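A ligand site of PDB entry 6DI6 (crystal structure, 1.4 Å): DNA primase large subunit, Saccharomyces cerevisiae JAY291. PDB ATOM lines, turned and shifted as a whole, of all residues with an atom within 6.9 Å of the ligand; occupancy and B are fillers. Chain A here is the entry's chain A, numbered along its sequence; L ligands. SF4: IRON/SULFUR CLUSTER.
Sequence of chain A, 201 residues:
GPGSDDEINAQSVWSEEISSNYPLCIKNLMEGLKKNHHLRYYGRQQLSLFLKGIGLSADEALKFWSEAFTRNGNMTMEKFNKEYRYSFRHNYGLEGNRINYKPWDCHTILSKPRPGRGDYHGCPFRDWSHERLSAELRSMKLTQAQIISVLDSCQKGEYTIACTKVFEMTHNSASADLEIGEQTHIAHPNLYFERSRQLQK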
ATOM      1  N   PRO A  23     -23.483  11.416  30.433  1.00  0.00           N
ATOM      2  CA  PRO A  23     -23.553  12.257  29.221  1.00  0.00           C
ATOM      3  C   PRO A  23     -22.908  13.609  29.487  1.00  0.00           C
ATOM      4  O   PRO A  23     -22.575  13.960  30.626  1.00  0.00           O
ATOM      5  CB  PRO A  23     -25.043  12.382  28.962  1.00  0.00           C
ATOM      6  CG  PRO A  23     -25.643  12.328  30.312  1.00  0.00           C
ATOM      7  CD  PRO A  23     -24.801  11.293  31.089  1.00  0.00           C
ATOM      8  N   LEU A  24     -22.772  14.410  28.424  1.00  0.00           N
ATOM      9  CA  LEU A  24     -21.972  15.632  28.538  1.00  0.00           C
ATOM     10  C   LEU A  24     -22.531  16.601  29.557  1.00  0.00           C
ATOM     11  O   LEU A  24     -21.776  17.285  30.249  1.00  0.00           O
ATOM     12  CB  LEU A  24     -21.820  16.379  27.199  1.00  0.00           C
ATOM     13  CG  LEU A  24     -20.852  15.823  26.175  1.00  0.00           C
ATOM     14  CD1 LEU A  24     -20.524  16.910  25.178  1.00  0.00           C
ATOM     15  CD2 LEU A  24     -19.595  15.298  26.852  1.00  0.00           C
ATOM     16  N   CYS A  25     -23.860  16.700  29.654  1.00  0.00           N
ATOM     17  CA  CYS A  25     -24.433  17.652  30.617  1.00  0.00           C
ATOM     18  C   CYS A  25     -24.033  17.301  32.059  1.00  0.00           C
ATOM     19  O   CYS A  25     -23.656  18.185  32.845  1.00  0.00           O
ATOM     20  CB  CYS A  25     -25.950  17.717  30.513  1.00  0.00           C
ATOM     21  SG  CYS A  25     -26.816  16.133  30.688  1.00  0.00           S
ATOM     22  N   ILE A  26     -24.095  15.999  32.409  1.00  0.00           N
ATOM     23  CA  ILE A  26     -23.711  15.547  33.749  1.00  0.00           C
ATOM     24  C   ILE A  26     -22.213  15.714  33.958  1.00  0.00           C
ATOM     25  O   ILE A  26     -21.769  16.127  35.031  1.00  0.00           O
ATOM     26  CB  ILE A  26     -24.206  14.113  33.976  1.00  0.00           C
ATOM     27  CG1 ILE A  26     -25.742  14.057  33.869  1.00  0.00           C
ATOM     28  CG2 ILE A  26     -23.735  13.556  35.315  1.00  0.00           C
ATOM     29  CD1 ILE A  26     -26.518  15.048  34.745  1.00  0.00           C
ATOM     30  N   GLN A  46     -30.558  19.696  38.554  1.00  0.00           N
ATOM     31  CA  GLN A  46     -30.314  18.779  37.437  1.00  0.00           C
ATOM     32  C   GLN A  46     -29.404  17.645  37.873  1.00  0.00           C
ATOM     33  O   GLN A  46     -29.698  16.461  37.625  1.00  0.00           O
ATOM     34  CB  GLN A  46     -29.686  19.536  36.282  1.00  0.00           C
ATOM     35  CG  GLN A  46     -29.507  18.688  35.015  1.00  0.00           C
ATOM     36  CD  GLN A  46     -29.080  19.512  33.805  1.00  0.00           C
ATOM     37  OE1 GLN A  46     -29.259  20.747  33.792  1.00  0.00           O
ATOM     38  NE2 GLN A  46     -28.499  18.831  32.779  1.00  0.00           N
ATOM     39  N   ASP A 105     -35.636  14.819  32.111  1.00  0.00           N
ATOM     40  CA  ASP A 105     -35.315  14.314  30.782  1.00  0.00           C
ATOM     41  C   ASP A 105     -34.708  15.434  29.933  1.00  0.00           C
ATOM     42  O   ASP A 105     -34.600  16.581  30.368  1.00  0.00           O
ATOM     43  CB  ASP A 105     -36.533  13.603  30.152  1.00  0.00           C
ATOM     44  CG  ASP A 105     -37.655  14.503  29.761  1.00  0.00           C
ATOM     45  OD1 ASP A 105     -37.542  15.725  29.844  1.00  0.00           O
ATOM     46  OD2 ASP A 105     -38.690  13.939  29.380  1.00  0.00           O
ATOM     47  N   CYS A 106     -34.292  15.113  28.706  1.00  0.00           N
ATOM     48  CA  CYS A 106     -33.593  16.107  27.897  1.00  0.00           C
ATOM     49  C   CYS A 106     -34.511  17.281  27.533  1.00  0.00           C
ATOM     50  O   CYS A 106     -34.091  18.440  27.549  1.00  0.00           O
ATOM     51  CB  CYS A 106     -33.033  15.500  26.617  1.00  0.00           C
ATOM     52  SG  CYS A 106     -31.791  14.207  26.964  1.00  0.00           S
ATOM     53  N   HIS A 107     -35.773  16.986  27.198  1.00  0.00           N
ATOM     54  CA  HIS A 107     -36.686  18.074  26.891  1.00  0.00           C
ATOM     55  C   HIS A 107     -36.861  19.018  28.074  1.00  0.00           C
ATOM     56  O   HIS A 107     -36.844  20.240  27.914  1.00  0.00           O
ATOM     57  CB  HIS A 107     -38.020  17.484  26.451  1.00  0.00           C
ATOM     58  CG  HIS A 107     -39.030  18.523  26.091  1.00  0.00           C
ATOM     59  ND1 HIS A 107     -39.056  19.157  24.873  1.00  0.00           N
ATOM     60  CD2 HIS A 107     -40.018  19.075  26.825  1.00  0.00           C
ATOM     61  CE1 HIS A 107     -40.048  20.046  24.863  1.00  0.00           C
ATOM     62  NE2 HIS A 107     -40.646  20.011  26.042  1.00  0.00           N
ATOM     63  N   ILE A 109     -34.674  19.497  30.519  1.00  0.00           N
ATOM     64  CA  ILE A 109     -33.419  20.229  30.667  1.00  0.00           C
ATOM     65  C   ILE A 109     -33.326  21.360  29.659  1.00  0.00           C
ATOM     66  O   ILE A 109     -32.985  22.493  30.015  1.00  0.00           O
ATOM     67  CB  ILE A 109     -32.247  19.266  30.523  1.00  0.00           C
ATOM     68  CG1 ILE A 109     -32.134  18.369  31.760  1.00  0.00           C
ATOM     69  CG2 ILE A 109     -30.940  20.020  30.254  1.00  0.00           C
ATOM     70  CD1 ILE A 109     -31.269  17.120  31.497  1.00  0.00           C
ATOM     71  N   LEU A 110     -33.627  21.062  28.387  1.00  0.00           N
ATOM     72  CA  LEU A 110     -33.546  22.075  27.337  1.00  0.00           C
ATOM     73  C   LEU A 110     -34.534  23.205  27.569  1.00  0.00           C
ATOM     74  O   LEU A 110     -34.308  24.334  27.128  1.00  0.00           O
ATOM     75  CB  LEU A 110     -33.751  21.439  25.938  1.00  0.00           C
ATOM     76  CG  LEU A 110     -32.571  20.596  25.456  1.00  0.00           C
ATOM     77  CD1 LEU A 110     -32.969  19.644  24.346  1.00  0.00           C
ATOM     78  CD2 LEU A 110     -31.425  21.480  24.982  1.00  0.00           C
ATOM     79  N   GLY A 122     -28.151  22.703  31.861  1.00  0.00           N
ATOM     80  CA  GLY A 122     -28.455  22.805  30.452  1.00  0.00           C
ATOM     81  C   GLY A 122     -27.896  21.621  29.684  1.00  0.00           C
ATOM     82  O   GLY A 122     -27.648  20.538  30.241  1.00  0.00           O
ATOM     83  N   CYS A 123     -27.695  21.835  28.390  1.00  0.00           N
ATOM     84  CA  CYS A 123     -27.230  20.801  27.461  1.00  0.00           C
ATOM     85  C   CYS A 123     -26.029  21.364  26.721  1.00  0.00           C
ATOM     86  O   CYS A 123     -26.186  22.291  25.915  1.00  0.00           O
ATOM     87  CB  CYS A 123     -28.338  20.462  26.459  1.00  0.00           C
ATOM     88  SG  CYS A 123     -27.747  19.275  25.218  1.00  0.00           S
ATOM     89  N   PRO A 124     -24.824  20.840  26.939  1.00  0.00           N
ATOM     90  CA  PRO A 124     -23.640  21.391  26.255  1.00  0.00           C
ATOM     91  C   PRO A 124     -23.727  21.376  24.737  1.00  0.00           C
ATOM     92  O   PRO A 124     -23.107  22.233  24.087  1.00  0.00           O
ATOM     93  CB  PRO A 124     -22.503  20.483  26.761  1.00  0.00           C
ATOM     94  CG  PRO A 124     -22.970  20.101  28.186  1.00  0.00           C
ATOM     95  CD  PRO A 124     -24.468  19.846  27.992  1.00  0.00           C
ATOM     96  N   PHE A 125     -24.462  20.448  24.124  1.00  0.00           N
ATOM     97  CA  PHE A 125     -24.530  20.457  22.662  1.00  0.00           C
ATOM     98  C   PHE A 125     -25.191  21.733  22.161  1.00  0.00           C
ATOM     99  O   PHE A 125     -24.930  22.144  21.024  1.00  0.00           O
ATOM    100  CB  PHE A 125     -25.254  19.210  22.173  1.00  0.00           C
ATOM    101  CG  PHE A 125     -24.504  17.973  22.490  1.00  0.00           C
ATOM    102  CD1 PHE A 125     -23.365  17.648  21.760  1.00  0.00           C
ATOM    103  CD2 PHE A 125     -24.891  17.134  23.523  1.00  0.00           C
ATOM    104  CE1 PHE A 125     -22.645  16.499  22.026  1.00  0.00           C
ATOM    105  CE2 PHE A 125     -24.163  15.986  23.821  1.00  0.00           C
ATOM    106  CZ  PHE A 125     -23.060  15.675  23.074  1.00  0.00           C
ATOM    107  N   ARG A 126     -26.040  22.363  22.968  1.00  0.00           N
ATOM    108  CA  ARG A 126     -26.612  23.668  22.649  1.00  0.00           C
ATOM    109  C   ARG A 126     -25.798  24.816  23.231  1.00  0.00           C
ATOM    110  O   ARG A 126     -25.605  25.850  22.582  1.00  0.00           O
ATOM    111  CB  ARG A 126     -28.033  23.771  23.219  1.00  0.00           C
ATOM    112  CG  ARG A 126     -28.699  25.120  22.915  1.00  0.00           C
ATOM    113  CD  ARG A 126     -29.996  25.237  23.693  1.00  0.00           C
ATOM    114  NE  ARG A 126     -29.698  25.277  25.131  1.00  0.00           N
ATOM    115  CZ  ARG A 126     -30.586  25.143  26.104  1.00  0.00           C
ATOM    116  NH1 ARG A 126     -31.886  25.041  25.826  1.00  0.00           N
ATOM    117  NH2 ARG A 126     -30.178  25.167  27.379  1.00  0.00           N
ATOM    118  N   TYR A 159     -30.073  18.510  19.317  1.00  0.00           N
ATOM    119  CA  TYR A 159     -29.121  18.271  20.404  1.00  0.00           C
ATOM    120  C   TYR A 159     -29.137  16.824  20.855  1.00  0.00           C
ATOM    121  O   TYR A 159     -28.082  16.259  21.164  1.00  0.00           O
ATOM    122  CB  TYR A 159     -29.395  19.230  21.589  1.00  0.00           C
ATOM    123  CG  TYR A 159     -29.449  20.649  21.072  1.00  0.00           C
ATOM    124  CD1 TYR A 159     -28.369  21.207  20.389  1.00  0.00           C
ATOM    125  CD2 TYR A 159     -30.596  21.400  21.237  1.00  0.00           C
ATOM    126  CE1 TYR A 159     -28.443  22.464  19.847  1.00  0.00           C
ATOM    127  CE2 TYR A 159     -30.674  22.691  20.717  1.00  0.00           C
ATOM    128  CZ  TYR A 159     -29.584  23.208  20.023  1.00  0.00           C
ATOM    129  OH  TYR A 159     -29.648  24.481  19.494  1.00  0.00           O
ATOM    130  N   THR A 160     -30.321  16.216  20.953  1.00  0.00           N
ATOM    131  CA  THR A 160     -30.367  14.835  21.413  1.00  0.00           C
ATOM    132  C   THR A 160     -29.811  13.874  20.363  1.00  0.00           C
ATOM    133  O   THR A 160     -29.286  12.819  20.731  1.00  0.00           O
ATOM    134  CB  THR A 160     -31.763  14.440  21.862  1.00  0.00           C
ATOM    135  OG1 THR A 160     -32.652  14.506  20.714  1.00  0.00           O
ATOM    136  CG2 THR A 160     -32.275  15.366  22.948  1.00  0.00           C
ATOM    137  N   ILE A 161     -29.891  14.231  19.076  1.00  0.00           N
ATOM    138  CA  ILE A 161     -29.199  13.442  18.054  1.00  0.00           C
ATOM    139  C   ILE A 161     -27.695  13.584  18.191  1.00  0.00           C
ATOM    140  O   ILE A 161     -26.962  12.592  18.092  1.00  0.00           O
ATOM    141  CB  ILE A 161     -29.705  13.806  16.644  1.00  0.00           C
ATOM    142  CG1 ILE A 161     -31.176  13.397  16.475  1.00  0.00           C
ATOM    143  CG2 ILE A 161     -28.871  13.114  15.584  1.00  0.00           C
ATOM    144  CD1 ILE A 161     -31.797  13.734  15.153  1.00  0.00           C
ATOM    145  N   ALA A 162     -27.210  14.816  18.428  1.00  0.00           N
ATOM    146  CA  ALA A 162     -25.782  15.011  18.666  1.00  0.00           C
ATOM    147  C   ALA A 162     -25.308  14.127  19.821  1.00  0.00           C
ATOM    148  O   ALA A 162     -24.267  13.453  19.732  1.00  0.00           O
ATOM    149  CB  ALA A 162     -25.528  16.474  18.967  1.00  0.00           C
ATOM    150  N   CYS A 163     -26.068  14.103  20.918  1.00  0.00           N
ATOM    151  CA  CYS A 163     -25.719  13.308  22.085  1.00  0.00           C
ATOM    152  C   CYS A 163     -25.745  11.815  21.745  1.00  0.00           C
ATOM    153  O   CYS A 163     -24.868  11.049  22.190  1.00  0.00           O
ATOM    154  CB  CYS A 163     -26.718  13.668  23.172  1.00  0.00           C
ATOM    155  SG  CYS A 163     -26.349  12.951  24.808  1.00  0.00           S
ATOM    156  N   THR A 164     -26.739  11.386  20.963  1.00  0.00           N
ATOM    157  CA  THR A 164     -26.800   9.988  20.551  1.00  0.00           C
ATOM    158  C   THR A 164     -25.594   9.608  19.697  1.00  0.00           C
ATOM    159  O   THR A 164     -25.035   8.522  19.855  1.00  0.00           O
ATOM    160  CB  THR A 164     -28.094   9.727  19.763  1.00  0.00           C
ATOM    161  OG1 THR A 164     -29.208  10.040  20.600  1.00  0.00           O
ATOM    162  CG2 THR A 164     -28.180   8.280  19.384  1.00  0.00           C
ATOM    163  N   ALA A 187     -35.610  10.772  25.067  1.00  0.00           N
ATOM    164  CA  ALA A 187     -34.262  11.268  25.320  1.00  0.00           C
ATOM    165  C   ALA A 187     -34.112  11.622  26.802  1.00  0.00           C
ATOM    166  O   ALA A 187     -34.874  12.452  27.343  1.00  0.00           O
ATOM    167  CB  ALA A 187     -34.060  12.526  24.474  1.00  0.00           C
ATOM    168  N   HIS A 188     -33.095  11.055  27.440  1.00  0.00           N
ATOM    169  CA  HIS A 188     -32.999  11.196  28.897  1.00  0.00           C
ATOM    170  C   HIS A 188     -31.579  10.957  29.359  1.00  0.00           C
ATOM    171  O   HIS A 188     -30.984   9.906  29.026  1.00  0.00           O
ATOM    172  CB  HIS A 188     -33.915  10.153  29.558  1.00  0.00           C
ATOM    173  CG  HIS A 188     -34.325  10.485  30.961  1.00  0.00           C
ATOM    174  ND1 HIS A 188     -33.410  10.739  31.981  1.00  0.00           N
ATOM    175  CD2 HIS A 188     -35.556  10.615  31.508  1.00  0.00           C
ATOM    176  CE1 HIS A 188     -34.077  11.002  33.085  1.00  0.00           C
ATOM    177  NE2 HIS A 188     -35.371  10.915  32.840  1.00  0.00           N
ATOM    178  N   PRO A 189     -30.974  11.889  30.131  1.00  0.00           N
ATOM    179  CA  PRO A 189     -29.611  11.630  30.642  1.00  0.00           C
ATOM    180  C   PRO A 189     -29.474  10.316  31.397  1.00  0.00           C
ATOM    181  O   PRO A 189     -28.431   9.649  31.329  1.00  0.00           O
ATOM    182  CB  PRO A 189     -29.338  12.821  31.550  1.00  0.00           C
ATOM    183  CG  PRO A 189     -30.273  13.878  31.094  1.00  0.00           C
ATOM    184  CD  PRO A 189     -31.520  13.171  30.601  1.00  0.00           C
ATOM    185  N   ASN A 190     -30.521   9.930  32.138  1.00  0.00           N
ATOM    186  CA  ASN A 190     -30.437   8.678  32.877  1.00  0.00           C
ATOM    187  C   ASN A 190     -30.445   7.464  31.957  1.00  0.00           C
ATOM    188  O   ASN A 190     -29.899   6.420  32.319  1.00  0.00           O
ATOM    189  CB  ASN A 190     -31.553   8.601  33.932  1.00  0.00           C
ATOM    190  CG  ASN A 190     -31.275   9.512  35.098  1.00  0.00           C
ATOM    191  OD1 ASN A 190     -31.522  10.705  35.028  1.00  0.00           O
ATOM    192  ND2 ASN A 190     -30.680   8.967  36.146  1.00  0.00           N
ATOM    193  N   TYR A 192     -29.013   7.521  28.930  1.00  0.00           N
ATOM    194  CA  TYR A 192     -27.630   7.494  28.471  1.00  0.00           C
ATOM    195  C   TYR A 192     -26.766   6.761  29.477  1.00  0.00           C
ATOM    196  O   TYR A 192     -26.026   5.835  29.139  1.00  0.00           O
ATOM    197  CB  TYR A 192     -27.141   8.932  28.305  1.00  0.00           C
ATOM    198  CG  TYR A 192     -25.804   9.126  27.596  1.00  0.00           C
ATOM    199  CD1 TYR A 192     -24.571   8.721  28.164  1.00  0.00           C
ATOM    200  CD2 TYR A 192     -25.782   9.770  26.347  1.00  0.00           C
ATOM    201  CE1 TYR A 192     -23.388   8.961  27.480  1.00  0.00           C
ATOM    202  CE2 TYR A 192     -24.610  10.000  25.691  1.00  0.00           C
ATOM    203  CZ  TYR A 192     -23.408   9.618  26.244  1.00  0.00           C
ATOM    204  OH  TYR A 192     -22.257   9.887  25.576  1.00  0.00           O
HETATM  205 FE1  SF4 L   1     -27.645  15.817  28.567  1.00  0.00          FE
HETATM  206 FE2  SF4 L   1     -29.783  15.254  26.963  1.00  0.00          FE
HETATM  207 FE3  SF4 L   1     -27.280  14.577  26.156  1.00  0.00          FE
HETATM  208 FE4  SF4 L   1     -28.016  17.210  26.231  1.00  0.00          FE
HETATM  209  S1  SF4 L   1     -28.890  15.643  24.896  1.00  0.00           S
HETATM  210  S2  SF4 L   1     -26.028  16.274  26.991  1.00  0.00           S
HETATM  211  S3  SF4 L   1     -29.420  17.198  28.042  1.00  0.00           S
HETATM  212  S4  SF4 L   1     -28.348  13.782  27.979  1.00  0.00           S
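SG of Cys 106 is bound to FE2 of the ligand (2.3 Å). The backbone NH (N) of Cys 25 lies close to a sulfur (S2) of the ligand (3.5 Å). FE1 of the ligand is bound by SG of Cys 25 (2.3 Å). The side-chain sulfur (SG) of Cys 163 is bound to an iron atom (FE3) of the ligand. The side-chain sulfur (SG) of Cys 123 binds an iron atom (FE4) of the ligand, 2.3 Å away.
N of His 188 sits close to SG of Cys 106 (3.4 Å). The backbone NH (N) of Cys 106 is in hydrogen-bond range of the backbone carbonyl oxygen (O) of Ala 187, at 3.0 Å. SG of Cys 123 sits close to N of Phe 125 (3.7 Å). The backbone carbonyl oxygen of Thr 160 lies within hydrogen-bond range of the side-chain hydroxyl of Thr 164 (2.8 Å).
CB of Pro 23 touches S4 of the ligand, 3.7 Å away. Ile 109 touches the ligand. Phe 125 touches the ligand. Tyr 159 touches the ligand (O to S1, 3.9 Å). Thr 160 touches the ligand. Pro 189 touches the ligand (CA to S4, 3.6 Å). Hydrophobic or aromatic side chains that line the ligand: Pro 23, Ile 109, Phe 125 and Pro 189. Ten residues have an atom within 4 Å of the ligand: Pro 23, Cys 25, Cys 106, Ile 109, Cys 123, Phe 125, Tyr 159, Thr 160, Cys 163 and Pro 189.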
